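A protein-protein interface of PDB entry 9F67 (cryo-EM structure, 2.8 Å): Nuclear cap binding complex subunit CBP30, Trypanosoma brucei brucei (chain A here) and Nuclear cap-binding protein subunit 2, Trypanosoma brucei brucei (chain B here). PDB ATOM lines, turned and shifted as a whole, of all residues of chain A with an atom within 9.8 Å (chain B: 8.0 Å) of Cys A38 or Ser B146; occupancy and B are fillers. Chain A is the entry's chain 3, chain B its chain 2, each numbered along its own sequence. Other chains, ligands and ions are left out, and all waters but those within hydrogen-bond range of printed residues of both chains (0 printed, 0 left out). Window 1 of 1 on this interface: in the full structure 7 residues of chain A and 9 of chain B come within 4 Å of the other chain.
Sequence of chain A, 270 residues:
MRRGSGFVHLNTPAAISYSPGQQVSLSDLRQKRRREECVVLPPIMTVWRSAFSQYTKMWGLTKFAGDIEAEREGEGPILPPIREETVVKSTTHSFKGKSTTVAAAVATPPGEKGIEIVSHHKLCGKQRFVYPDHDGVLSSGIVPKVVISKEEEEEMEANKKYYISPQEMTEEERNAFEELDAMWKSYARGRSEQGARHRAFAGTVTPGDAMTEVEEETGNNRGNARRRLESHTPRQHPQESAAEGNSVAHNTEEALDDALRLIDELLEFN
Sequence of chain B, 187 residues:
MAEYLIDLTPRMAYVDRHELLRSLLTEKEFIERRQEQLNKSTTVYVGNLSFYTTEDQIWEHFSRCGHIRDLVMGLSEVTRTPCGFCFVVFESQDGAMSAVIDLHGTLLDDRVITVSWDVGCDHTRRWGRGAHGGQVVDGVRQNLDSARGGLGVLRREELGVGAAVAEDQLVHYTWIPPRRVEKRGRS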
ATOM      1  N   LEU A  29      -4.962   7.528   2.536  1.00  0.00           N
ATOM      2  CA  LEU A  29      -5.492   6.537   3.464  1.00  0.00           C
ATOM      3  C   LEU A  29      -5.327   7.029   4.895  1.00  0.00           C
ATOM      4  O   LEU A  29      -4.291   6.790   5.524  1.00  0.00           O
ATOM      5  CB  LEU A  29      -4.798   5.186   3.277  1.00  0.00           C
ATOM      6  CG  LEU A  29      -5.223   4.307   2.095  1.00  0.00           C
ATOM      7  CD1 LEU A  29      -4.726   4.862   0.766  1.00  0.00           C
ATOM      8  CD2 LEU A  29      -4.740   2.877   2.293  1.00  0.00           C
ATOM      9  N   ARG A  30      -6.338   7.724   5.414  1.00  0.00           N
ATOM     10  CA  ARG A  30      -6.277   8.341   6.735  1.00  0.00           C
ATOM     11  C   ARG A  30      -7.461   7.858   7.560  1.00  0.00           C
ATOM     12  O   ARG A  30      -8.616   8.048   7.165  1.00  0.00           O
ATOM     13  CB  ARG A  30      -6.276   9.866   6.625  1.00  0.00           C
ATOM     14  CG  ARG A  30      -5.213  10.414   5.692  1.00  0.00           C
ATOM     15  CD  ARG A  30      -4.893  11.862   6.016  1.00  0.00           C
ATOM     16  NE  ARG A  30      -4.703  12.068   7.447  1.00  0.00           N
ATOM     17  CZ  ARG A  30      -3.573  11.825   8.096  1.00  0.00           C
ATOM     18  NH1 ARG A  30      -2.502  11.363   7.471  1.00  0.00           N
ATOM     19  NH2 ARG A  30      -3.515  12.049   9.405  1.00  0.00           N
ATOM     20  N   GLN A  31      -7.177   7.240   8.701  1.00  0.00           N
ATOM     21  CA  GLN A  31      -8.212   6.766   9.613  1.00  0.00           C
ATOM     22  C   GLN A  31      -7.784   7.137  11.028  1.00  0.00           C
ATOM     23  O   GLN A  31      -6.844   7.911  11.237  1.00  0.00           O
ATOM     24  CB  GLN A  31      -8.454   5.254   9.452  1.00  0.00           C
ATOM     25  CG  GLN A  31      -8.598   4.759   8.016  1.00  0.00           C
ATOM     26  CD  GLN A  31      -7.261   4.515   7.341  1.00  0.00           C
ATOM     27  OE1 GLN A  31      -6.205   4.796   7.908  1.00  0.00           O
ATOM     28  NE2 GLN A  31      -7.302   3.987   6.123  1.00  0.00           N
ATOM     29  N   LYS A  32      -8.482   6.589  12.020  1.00  0.00           N
ATOM     30  CA  LYS A  32      -8.105   6.803  13.409  1.00  0.00           C
ATOM     31  C   LYS A  32      -6.780   6.116  13.709  1.00  0.00           C
ATOM     32  O   LYS A  32      -6.519   5.004  13.242  1.00  0.00           O
ATOM     33  CB  LYS A  32      -9.195   6.281  14.344  1.00  0.00           C
ATOM     34  CG  LYS A  32     -10.553   6.933  14.136  1.00  0.00           C
ATOM     35  CD  LYS A  32     -10.453   8.448  14.182  1.00  0.00           C
ATOM     36  CE  LYS A  32     -10.973   9.074  12.899  1.00  0.00           C
ATOM     37  NZ  LYS A  32     -10.846  10.558  12.913  1.00  0.00           N
ATOM     38  N   ARG A  33      -5.938   6.784  14.500  1.00  0.00           N
ATOM     39  CA  ARG A  33      -4.596   6.297  14.792  1.00  0.00           C
ATOM     40  C   ARG A  33      -4.406   5.962  16.265  1.00  0.00           C
ATOM     41  O   ARG A  33      -3.266   5.794  16.712  1.00  0.00           O
ATOM     42  CB  ARG A  33      -3.549   7.321  14.348  1.00  0.00           C
ATOM     43  CG  ARG A  33      -3.647   7.714  12.888  1.00  0.00           C
ATOM     44  CD  ARG A  33      -2.329   8.269  12.384  1.00  0.00           C
ATOM     45  NE  ARG A  33      -1.233   7.330  12.585  1.00  0.00           N
ATOM     46  CZ  ARG A  33       0.029   7.574  12.258  1.00  0.00           C
ATOM     47  NH1 ARG A  33       0.393   8.723  11.712  1.00  0.00           N
ATOM     48  NH2 ARG A  33       0.949   6.640  12.484  1.00  0.00           N
ATOM     49  N   ARG A  34      -5.494   5.854  17.025  1.00  0.00           N
ATOM     50  CA  ARG A  34      -5.454   5.558  18.463  1.00  0.00           C
ATOM     51  C   ARG A  34      -4.569   6.611  19.129  1.00  0.00           C
ATOM     52  O   ARG A  34      -4.628   7.786  18.740  1.00  0.00           O
ATOM     53  CB  ARG A  34      -5.021   4.114  18.671  1.00  0.00           C
ATOM     54  CG  ARG A  34      -5.805   3.379  19.740  1.00  0.00           C
ATOM     55  CD  ARG A  34      -5.665   1.872  19.590  1.00  0.00           C
ATOM     56  NE  ARG A  34      -4.284   1.474  19.344  1.00  0.00           N
ATOM     57  CZ  ARG A  34      -3.889   0.223  19.148  1.00  0.00           C
ATOM     58  NH1 ARG A  34      -4.748  -0.784  19.162  1.00  0.00           N
ATOM     59  NH2 ARG A  34      -2.600  -0.024  18.933  1.00  0.00           N
ATOM     60  N   ARG A  35      -3.724   6.193  20.077  1.00  0.00           N
ATOM     61  CA  ARG A  35      -2.782   7.146  20.724  1.00  0.00           C
ATOM     62  C   ARG A  35      -1.365   6.546  20.736  1.00  0.00           C
ATOM     63  O   ARG A  35      -0.392   7.321  20.601  1.00  0.00           O
ATOM     64  CB  ARG A  35      -3.234   7.490  22.150  1.00  0.00           C
ATOM     65  CG  ARG A  35      -2.392   8.580  22.799  1.00  0.00           C
ATOM     66  CD  ARG A  35      -2.780   8.857  24.243  1.00  0.00           C
ATOM     67  NE  ARG A  35      -1.902   9.860  24.855  1.00  0.00           N
ATOM     68  CZ  ARG A  35      -1.994  10.284  26.108  1.00  0.00           C
ATOM     69  NH1 ARG A  35      -2.909   9.775  26.914  1.00  0.00           N
ATOM     70  NH2 ARG A  35      -1.169  11.215  26.554  1.00  0.00           N
ATOM     71  N   GLU A  36      -1.255   5.221  20.876  1.00  0.00           N
ATOM     72  CA  GLU A  36       0.077   4.564  20.964  1.00  0.00           C
ATOM     73  C   GLU A  36       0.631   4.294  19.554  1.00  0.00           C
ATOM     74  O   GLU A  36       1.734   3.715  19.456  1.00  0.00           O
ATOM     75  CB  GLU A  36      -0.035   3.270  21.772  1.00  0.00           C
ATOM     76  CG  GLU A  36      -1.281   2.460  21.431  1.00  0.00           C
ATOM     77  CD  GLU A  36      -1.323   1.094  22.092  1.00  0.00           C
ATOM     78  OE1 GLU A  36      -0.343   0.746  22.783  1.00  0.00           O
ATOM     79  OE2 GLU A  36      -2.335   0.383  21.924  1.00  0.00           O
ATOM     80  N   GLU A  37      -0.105   4.694  18.513  1.00  0.00           N
ATOM     81  CA  GLU A  37       0.347   4.477  17.112  1.00  0.00           C
ATOM     82  C   GLU A  37       0.721   5.834  16.496  1.00  0.00           C
ATOM     83  O   GLU A  37       1.153   5.859  15.323  1.00  0.00           O
ATOM     84  CB  GLU A  37      -0.759   3.750  16.348  1.00  0.00           C
ATOM     85  CG  GLU A  37      -0.295   3.117  15.039  1.00  0.00           C
ATOM     86  CD  GLU A  37      -0.704   3.884  13.795  1.00  0.00           C
ATOM     87  OE1 GLU A  37      -1.389   4.917  13.936  1.00  0.00           O
ATOM     88  OE2 GLU A  37      -0.333   3.451  12.684  1.00  0.00           O
ATOM     89  N   CYS A  38       0.586   6.918  17.266  1.00  0.00           N
ATOM     90  CA  CYS A  38       0.875   8.250  16.753  1.00  0.00           C
ATOM     91  C   CYS A  38       2.082   8.882  17.434  1.00  0.00           C
ATOM     92  O   CYS A  38       2.268  10.100  17.334  1.00  0.00           O
ATOM     93  CB  CYS A  38      -0.340   9.163  16.917  1.00  0.00           C
ATOM     94  SG  CYS A  38      -0.678   9.640  18.619  1.00  0.00           S
ATOM     95  N   VAL A  39       2.950   8.030  18.008  1.00  0.00           N
ATOM     96  CA  VAL A  39       4.166   8.411  18.775  1.00  0.00           C
ATOM     97  C   VAL A  39       5.388   8.219  17.907  1.00  0.00           C
ATOM     98  O   VAL A  39       5.764   7.090  17.684  1.00  0.00           O
ATOM     99  CB  VAL A  39       4.398   7.619  20.064  1.00  0.00           C
ATOM    100  CG1 VAL A  39       3.539   8.151  21.197  1.00  0.00           C
ATOM    101  CG2 VAL A  39       4.137   6.140  19.892  1.00  0.00           C
ATOM    102  N   VAL A  40       6.032   9.305  17.519  1.00  0.00           N
ATOM    103  CA  VAL A  40       7.261   9.106  16.765  1.00  0.00           C
ATOM    104  C   VAL A  40       8.422   9.654  17.579  1.00  0.00           C
ATOM    105  O   VAL A  40       8.411  10.816  17.999  1.00  0.00           O
ATOM    106  CB  VAL A  40       7.166   9.777  15.390  1.00  0.00           C
ATOM    107  CG1 VAL A  40       8.260   9.277  14.494  1.00  0.00           C
ATOM    108  CG2 VAL A  40       5.819   9.494  14.769  1.00  0.00           C
ATOM    109  N   LEU A  41       9.418   8.828  17.799  1.00  0.00           N
ATOM    110  CA  LEU A  41      10.486   9.054  18.754  1.00  0.00           C
ATOM    111  C   LEU A  41      11.602   9.895  18.150  1.00  0.00           C
ATOM    112  O   LEU A  41      11.733   9.989  16.927  1.00  0.00           O
ATOM    113  CB  LEU A  41      11.033   7.708  19.233  1.00  0.00           C
ATOM    114  CG  LEU A  41      10.186   7.060  20.324  1.00  0.00           C
ATOM    115  CD1 LEU A  41      10.860   5.815  20.849  1.00  0.00           C
ATOM    116  CD2 LEU A  41       9.936   8.036  21.447  1.00  0.00           C
ATOM    117  N   ILE A  78       7.419  -1.413  18.844  1.00  0.00           N
ATOM    118  CA  ILE A  78       8.165  -0.266  19.394  1.00  0.00           C
ATOM    119  C   ILE A  78       8.065   0.852  18.401  1.00  0.00           C
ATOM    120  O   ILE A  78       8.287   0.609  17.235  1.00  0.00           O
ATOM    121  CB  ILE A  78       9.581  -0.633  19.891  1.00  0.00           C
ATOM    122  CG1 ILE A  78      10.426  -1.277  18.795  1.00  0.00           C
ATOM    123  CG2 ILE A  78       9.531  -1.519  21.121  1.00  0.00           C
ATOM    124  CD1 ILE A  78      11.804  -1.677  19.258  1.00  0.00           C
ATOM    125  N   LEU A  79       7.872   2.048  18.957  1.00  0.00           N
ATOM    126  CA  LEU A  79       7.590   3.281  18.194  1.00  0.00           C
ATOM    127  C   LEU A  79       8.658   3.623  17.168  1.00  0.00           C
ATOM    128  O   LEU A  79       9.850   3.380  17.432  1.00  0.00           O
ATOM    129  CB  LEU A  79       7.641   4.394  19.241  1.00  0.00           C
ATOM    130  CG  LEU A  79       7.087   4.071  20.630  1.00  0.00           C
ATOM    131  CD1 LEU A  79       7.006   5.338  21.457  1.00  0.00           C
ATOM    132  CD2 LEU A  79       5.737   3.363  20.590  1.00  0.00           C
ATOM    133  N   PRO A  80       8.327   4.301  16.032  1.00  0.00           N
ATOM    134  CA  PRO A  80       9.339   4.704  15.038  1.00  0.00           C
ATOM    135  C   PRO A  80      10.198   5.931  15.385  1.00  0.00           C
ATOM    136  O   PRO A  80       9.698   6.842  16.012  1.00  0.00           O
ATOM    137  CB  PRO A  80       8.514   5.039  13.785  1.00  0.00           C
ATOM    138  CG  PRO A  80       7.222   5.573  14.339  1.00  0.00           C
ATOM    139  CD  PRO A  80       6.983   4.730  15.573  1.00  0.00           C
ATOM    140  N   ILE A  82      12.549   9.317  14.227  1.00  0.00           N
ATOM    141  CA  ILE A  82      12.349  10.123  12.983  1.00  0.00           C
ATOM    142  C   ILE A  82      13.645  10.121  12.157  1.00  0.00           C
ATOM    143  O   ILE A  82      14.722   9.932  12.769  1.00  0.00           O
ATOM    144  CB  ILE A  82      11.900  11.559  13.314  1.00  0.00           C
ATOM    145  CG1 ILE A  82      13.062  12.422  13.800  1.00  0.00           C
ATOM    146  CG2 ILE A  82      10.744  11.562  14.314  1.00  0.00           C
ATOM    147  CD1 ILE A  82      12.666  13.838  14.173  1.00  0.00           C
ATOM    148  N   SER B  50       1.159  17.093  22.613  1.00  0.00           N
ATOM    149  CA  SER B  50       0.042  16.402  21.919  1.00  0.00           C
ATOM    150  C   SER B  50      -1.280  16.829  22.563  1.00  0.00           C
ATOM    151  O   SER B  50      -1.302  17.009  23.794  1.00  0.00           O
ATOM    152  CB  SER B  50       0.210  14.909  21.965  1.00  0.00           C
ATOM    153  OG  SER B  50       0.223  14.442  23.305  1.00  0.00           O
ATOM    154  N   PHE B  51      -2.334  17.001  21.765  1.00  0.00           N
ATOM    155  CA  PHE B  51      -3.659  17.316  22.358  1.00  0.00           C
ATOM    156  C   PHE B  51      -3.931  16.226  23.397  1.00  0.00           C
ATOM    157  O   PHE B  51      -4.668  16.485  24.367  1.00  0.00           O
ATOM    158  CB  PHE B  51      -4.724  17.403  21.261  1.00  0.00           C
ATOM    159  CG  PHE B  51      -4.492  18.459  20.206  1.00  0.00           C
ATOM    160  CD1 PHE B  51      -3.387  19.296  20.248  1.00  0.00           C
ATOM    161  CD2 PHE B  51      -5.380  18.607  19.153  1.00  0.00           C
ATOM    162  CE1 PHE B  51      -3.178  20.253  19.268  1.00  0.00           C
ATOM    163  CE2 PHE B  51      -5.172  19.567  18.176  1.00  0.00           C
ATOM    164  CZ  PHE B  51      -4.072  20.390  18.234  1.00  0.00           C
ATOM    165  N   TYR B  52      -3.341  15.045  23.194  1.00  0.00           N
ATOM    166  CA  TYR B  52      -3.454  13.922  24.158  1.00  0.00           C
ATOM    167  C   TYR B  52      -2.743  14.256  25.475  1.00  0.00           C
ATOM    168  O   TYR B  52      -3.257  13.841  26.529  1.00  0.00           O
ATOM    169  CB  TYR B  52      -2.834  12.668  23.544  1.00  0.00           C
ATOM    170  CG  TYR B  52      -3.480  12.205  22.264  1.00  0.00           C
ATOM    171  CD1 TYR B  52      -4.812  11.829  22.233  1.00  0.00           C
ATOM    172  CD2 TYR B  52      -2.757  12.126  21.086  1.00  0.00           C
ATOM    173  CE1 TYR B  52      -5.413  11.395  21.063  1.00  0.00           C
ATOM    174  CE2 TYR B  52      -3.343  11.697  19.907  1.00  0.00           C
ATOM    175  CZ  TYR B  52      -4.675  11.330  19.896  1.00  0.00           C
ATOM    176  OH  TYR B  52      -5.266  10.901  18.732  1.00  0.00           O
ATOM    177  N   ASP B 109       5.758  14.055  26.885  1.00  0.00           N
ATOM    178  CA  ASP B 109       4.896  12.920  26.462  1.00  0.00           C
ATOM    179  C   ASP B 109       5.435  12.392  25.128  1.00  0.00           C
ATOM    180  O   ASP B 109       4.746  12.581  24.104  1.00  0.00           O
ATOM    181  CB  ASP B 109       3.425  13.347  26.410  1.00  0.00           C
ATOM    182  CG  ASP B 109       2.434  12.225  26.140  1.00  0.00           C
ATOM    183  OD1 ASP B 109       2.873  11.065  25.994  1.00  0.00           O
ATOM    184  OD2 ASP B 109       1.225  12.522  26.073  1.00  0.00           O
ATOM    185  N   ASP B 110       6.626  11.789  25.131  1.00  0.00           N
ATOM    186  CA  ASP B 110       7.184  11.169  23.897  1.00  0.00           C
ATOM    187  C   ASP B 110       7.243  12.200  22.762  1.00  0.00           C
ATOM    188  O   ASP B 110       6.952  11.813  21.612  1.00  0.00           O
ATOM    189  CB  ASP B 110       6.380   9.931  23.497  1.00  0.00           C
ATOM    190  CG  ASP B 110       6.268   8.938  24.639  1.00  0.00           C
ATOM    191  OD1 ASP B 110       7.324   8.485  25.116  1.00  0.00           O
ATOM    192  OD2 ASP B 110       5.128   8.627  25.038  1.00  0.00           O
ATOM    193  N   ARG B 111       7.615  13.447  23.069  1.00  0.00           N
ATOM    194  CA  ARG B 111       7.681  14.521  22.039  1.00  0.00           C
ATOM    195  C   ARG B 111       8.578  15.647  22.558  1.00  0.00           C
ATOM    196  O   ARG B 111       8.589  15.869  23.782  1.00  0.00           O
ATOM    197  CB  ARG B 111       6.271  15.012  21.701  1.00  0.00           C
ATOM    198  CG  ARG B 111       5.514  15.591  22.886  1.00  0.00           C
ATOM    199  CD  ARG B 111       4.102  15.917  22.457  1.00  0.00           C
ATOM    200  NE  ARG B 111       4.028  16.875  21.363  1.00  0.00           N
ATOM    201  CZ  ARG B 111       3.471  16.622  20.186  1.00  0.00           C
ATOM    202  NH1 ARG B 111       3.205  17.611  19.352  1.00  0.00           N
ATOM    203  NH2 ARG B 111       3.132  15.386  19.869  1.00  0.00           N
ATOM    204  N   ARG B 141       1.247  24.872   9.209  1.00  0.00           N
ATOM    205  CA  ARG B 141       2.169  23.710   9.203  1.00  0.00           C
ATOM    206  C   ARG B 141       1.928  22.821   7.992  1.00  0.00           C
ATOM    207  O   ARG B 141       0.785  22.687   7.589  1.00  0.00           O
ATOM    208  CB  ARG B 141       2.039  22.934  10.508  1.00  0.00           C
ATOM    209  CG  ARG B 141       0.685  22.338  10.826  1.00  0.00           C
ATOM    210  CD  ARG B 141       0.950  21.548  12.085  1.00  0.00           C
ATOM    211  NE  ARG B 141      -0.237  20.858  12.538  1.00  0.00           N
ATOM    212  CZ  ARG B 141      -0.301  19.542  12.613  1.00  0.00           C
ATOM    213  NH1 ARG B 141      -1.366  18.948  13.121  1.00  0.00           N
ATOM    214  NH2 ARG B 141       0.704  18.827  12.144  1.00  0.00           N
ATOM    215  N   ASN B 143       3.059  19.508   7.558  1.00  0.00           N
ATOM    216  CA  ASN B 143       3.636  18.181   7.913  1.00  0.00           C
ATOM    217  C   ASN B 143       2.544  17.269   8.478  1.00  0.00           C
ATOM    218  O   ASN B 143       1.438  17.776   8.766  1.00  0.00           O
ATOM    219  CB  ASN B 143       4.773  18.323   8.918  1.00  0.00           C
ATOM    220  CG  ASN B 143       6.008  18.937   8.301  1.00  0.00           C
ATOM    221  OD1 ASN B 143       6.189  18.875   7.079  1.00  0.00           O
ATOM    222  ND2 ASN B 143       6.865  19.531   9.119  1.00  0.00           N
ATOM    223  N   LEU B 144       2.843  15.974   8.631  1.00  0.00           N
ATOM    224  CA  LEU B 144       1.869  15.060   9.261  1.00  0.00           C
ATOM    225  C   LEU B 144       2.269  14.844  10.734  1.00  0.00           C
ATOM    226  O   LEU B 144       2.978  13.859  11.015  1.00  0.00           O
ATOM    227  CB  LEU B 144       1.752  13.741   8.501  1.00  0.00           C
ATOM    228  CG  LEU B 144       1.188  13.814   7.080  1.00  0.00           C
ATOM    229  CD1 LEU B 144       1.282  12.445   6.432  1.00  0.00           C
ATOM    230  CD2 LEU B 144      -0.258  14.286   7.091  1.00  0.00           C
ATOM    231  N   ASP B 145       1.770  15.697  11.635  1.00  0.00           N
ATOM    232  CA  ASP B 145       1.989  15.474  13.092  1.00  0.00           C
ATOM    233  C   ASP B 145       0.665  14.942  13.648  1.00  0.00           C
ATOM    234  O   ASP B 145      -0.175  15.772  14.059  1.00  0.00           O
ATOM    235  CB  ASP B 145       2.496  16.728  13.786  1.00  0.00           C
ATOM    236  CG  ASP B 145       2.925  16.547  15.237  1.00  0.00           C
ATOM    237  OD1 ASP B 145       2.812  15.413  15.748  1.00  0.00           O
ATOM    238  OD2 ASP B 145       3.375  17.543  15.843  1.00  0.00           O
ATOM    239  N   SER B 146       0.462  13.621  13.602  1.00  0.00           N
ATOM    240  CA  SER B 146      -0.835  13.021  14.019  1.00  0.00           C
ATOM    241  C   SER B 146      -1.227  13.454  15.438  1.00  0.00           C
ATOM    242  O   SER B 146      -2.433  13.687  15.668  1.00  0.00           O
ATOM    243  CB  SER B 146      -0.790  11.517  13.904  1.00  0.00           C
ATOM    244  OG  SER B 146      -0.499  11.124  12.571  1.00  0.00           O
ATOM    245  N   ALA B 147      -0.290  13.595  16.342  1.00  0.00           N
ATOM    246  CA  ALA B 147      -0.647  13.896  17.732  1.00  0.00           C
ATOM    247  C   ALA B 147      -1.194  15.300  17.827  1.00  0.00           C
ATOM    248  O   ALA B 147      -1.820  15.600  18.841  1.00  0.00           O
ATOM    249  CB  ALA B 147       0.570  13.743  18.579  1.00  0.00           C
ATOM    250  N   ARG B 148      -0.909  16.143  16.857  1.00  0.00           N
ATOM    251  CA  ARG B 148      -1.527  17.496  16.819  1.00  0.00           C
ATOM    252  C   ARG B 148      -2.777  17.451  15.923  1.00  0.00           C
ATOM    253  O   ARG B 148      -3.245  18.533  15.507  1.00  0.00           O
ATOM    254  CB  ARG B 148      -0.521  18.549  16.339  1.00  0.00           C
ATOM    255  CG  ARG B 148       0.627  18.770  17.314  1.00  0.00           C
ATOM    256  CD  ARG B 148       1.471  19.982  16.949  1.00  0.00           C
ATOM    257  NE  ARG B 148       0.812  21.265  17.221  1.00  0.00           N
ATOM    258  CZ  ARG B 148       0.488  21.725  18.426  1.00  0.00           C
ATOM    259  NH1 ARG B 148      -0.309  22.772  18.539  1.00  0.00           N
ATOM    260  NH2 ARG B 148       0.962  21.140  19.512  1.00  0.00           N
ATOM    261  N   GLY B 149      -3.287  16.248  15.639  1.00  0.00           N
ATOM    262  CA  GLY B 149      -4.502  16.104  14.813  1.00  0.00           C
ATOM    263  C   GLY B 149      -4.171  15.593  13.424  1.00  0.00           C
ATOM    264  O   GLY B 149      -5.110  15.205  12.701  1.00  0.00           O
ATOM    265  N   GLY B 150      -2.973  15.824  12.938  1.00  0.00           N
ATOM    266  CA  GLY B 150      -2.708  15.453  11.547  1.00  0.00           C
ATOM    267  C   GLY B 150      -2.071  16.577  10.773  1.00  0.00           C
ATOM    268  O   GLY B 150      -1.090  17.126  11.239  1.00  0.00           O
ATOM    269  N   LEU B 151      -2.583  16.855   9.597  1.00  0.00           N
ATOM    270  CA  LEU B 151      -2.028  17.924   8.758  1.00  0.00           C
ATOM    271  C   LEU B 151      -2.555  19.217   9.348  1.00  0.00           C
ATOM    272  O   LEU B 151      -3.365  19.175  10.265  1.00  0.00           O
ATOM    273  CB  LEU B 151      -2.493  17.812   7.309  1.00  0.00           C
ATOM    274  CG  LEU B 151      -2.369  16.493   6.565  1.00  0.00           C
ATOM    275  CD1 LEU B 151      -3.555  15.580   6.846  1.00  0.00           C
ATOM    276  CD2 LEU B 151      -2.199  16.727   5.074  1.00  0.00           C
ATOM    277  N   ARG B 156      -5.182  20.453   5.538  1.00  0.00           N
ATOM    278  CA  ARG B 156      -6.287  19.487   5.662  1.00  0.00           C
ATOM    279  C   ARG B 156      -7.553  20.033   5.039  1.00  0.00           C
ATOM    280  O   ARG B 156      -8.218  19.261   4.326  1.00  0.00           O
ATOM    281  CB  ARG B 156      -6.749  19.220   7.093  1.00  0.00           C
ATOM    282  CG  ARG B 156      -5.701  18.567   7.976  1.00  0.00           C
ATOM    283  CD  ARG B 156      -6.140  18.153   9.366  1.00  0.00           C
ATOM    284  NE  ARG B 156      -7.118  17.077   9.388  1.00  0.00           N
ATOM    285  CZ  ARG B 156      -7.618  16.557  10.502  1.00  0.00           C
ATOM    286  NH1 ARG B 156      -8.410  15.502  10.445  1.00  0.00           N
ATOM    287  NH2 ARG B 156      -7.290  17.070  11.676  1.00  0.00           N
ATOM    288  N   GLU B 167     -12.089  15.458  18.834  1.00  0.00           N
ATOM    289  CA  GLU B 167     -12.413  14.050  19.029  1.00  0.00           C
ATOM    290  C   GLU B 167     -13.031  13.826  20.402  1.00  0.00           C
ATOM    291  O   GLU B 167     -13.453  14.774  21.062  1.00  0.00           O
ATOM    292  CB  GLU B 167     -11.165  13.185  18.854  1.00  0.00           C
ATOM    293  CG  GLU B 167     -10.192  13.724  17.819  1.00  0.00           C
ATOM    294  CD  GLU B 167      -9.147  12.707  17.409  1.00  0.00           C
ATOM    295  OE1 GLU B 167      -9.247  11.540  17.843  1.00  0.00           O
ATOM    296  OE2 GLU B 167      -8.224  13.076  16.653  1.00  0.00           O
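OD2 of Asp B109 is in salt-bridge range of NH2 of Arg A35.
The guanidinium group of Arg A35 is in hydrogen-bond range of the backbone carbonyl oxygen of Tyr B52 (3.4 Å).
The side-chain hydroxyl (OH) of Tyr B52 lies within hydrogen-bond range of the backbone carbonyl oxygen (O) of Arg A34.
The guanidinium group of Arg A33 lies within hydrogen-bond range of the side-chain hydroxyl of Ser B146 (2.7 Å).
NE of Arg A33 is in salt-bridge range of OE1 of Glu A37 (2.8 Å).
The guanidinium group of Arg A34 lies within salt-bridge range of the side-chain carboxylate of Glu A36, 3.0 Å away.
NH1 of Arg B141 is in hydrogen-bond range of O of Leu B151 (3.5 Å).
SG of Cys A38 is in hydrogen-bond range of O of Arg A35, at 3.1 Å.
Among the printed residues, merely in contact across the chains: Arg A30 with Leu B144, Arg A30 with Leu B151, Cys A38 with Tyr B52 and Cys A38 with Ser B146.
Leu A29 touches none of the printed residues of chain B.
Printed residues of chain B within 4 Å of Arg A30: Leu B144 and Leu B151.
Of the printed residues of chain B, Arg A33 touches Ser B146 (2.7 Å).
Glu A36 touches none of the printed residues of chain B.
Cys A38 touches just these residues of chain B: Tyr B52 (3.6 Å) and Ser B146 (3.8 Å).
Of the printed residues of chain A, Asp B109 touches Arg A35 (2.8 Å).
Printed residues of chain A within 4 Å of Leu B144: Arg A30 (3.7 Å).
Printed residues of chain A within 4 Å of Ser B146: Arg A33 and Cys A38.
No residue of chain A comes within 4 Å of Ala B147.
No residue of chain A comes within 4 Å of Gly B149.
No residue of chain A comes within 4 Å of Gly B150.
Of the printed residues of chain A, Leu B151 touches Arg A30 (3.7 Å).
The nearest printed residue of chain A that does not touch Asp B109 is Val A39 (5.4 Å).
Printed residues of chain A that touch a printed residue of chain B: Arg A30, Arg A33, Arg A34, Arg A35 and Cys A38.
Printed residues of chain B that touch a printed residue of chain A: Tyr B52, Asp B109, Leu B144, Ser B146 and Leu B151.
Hydrophobic or aromatic side chains of chain B that line the printed part of chain A: Tyr B52, Leu B144 and Leu B151.
Along chain B the printed residues that touch a printed residue of chain A span positions 52 to 151.
Among the printed residues, Asp or Glu carboxylates within 4 Å of a Lys or Arg side-chain nitrogen of the other chain: Arg A35 with Asp B109 (2.8 Å).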
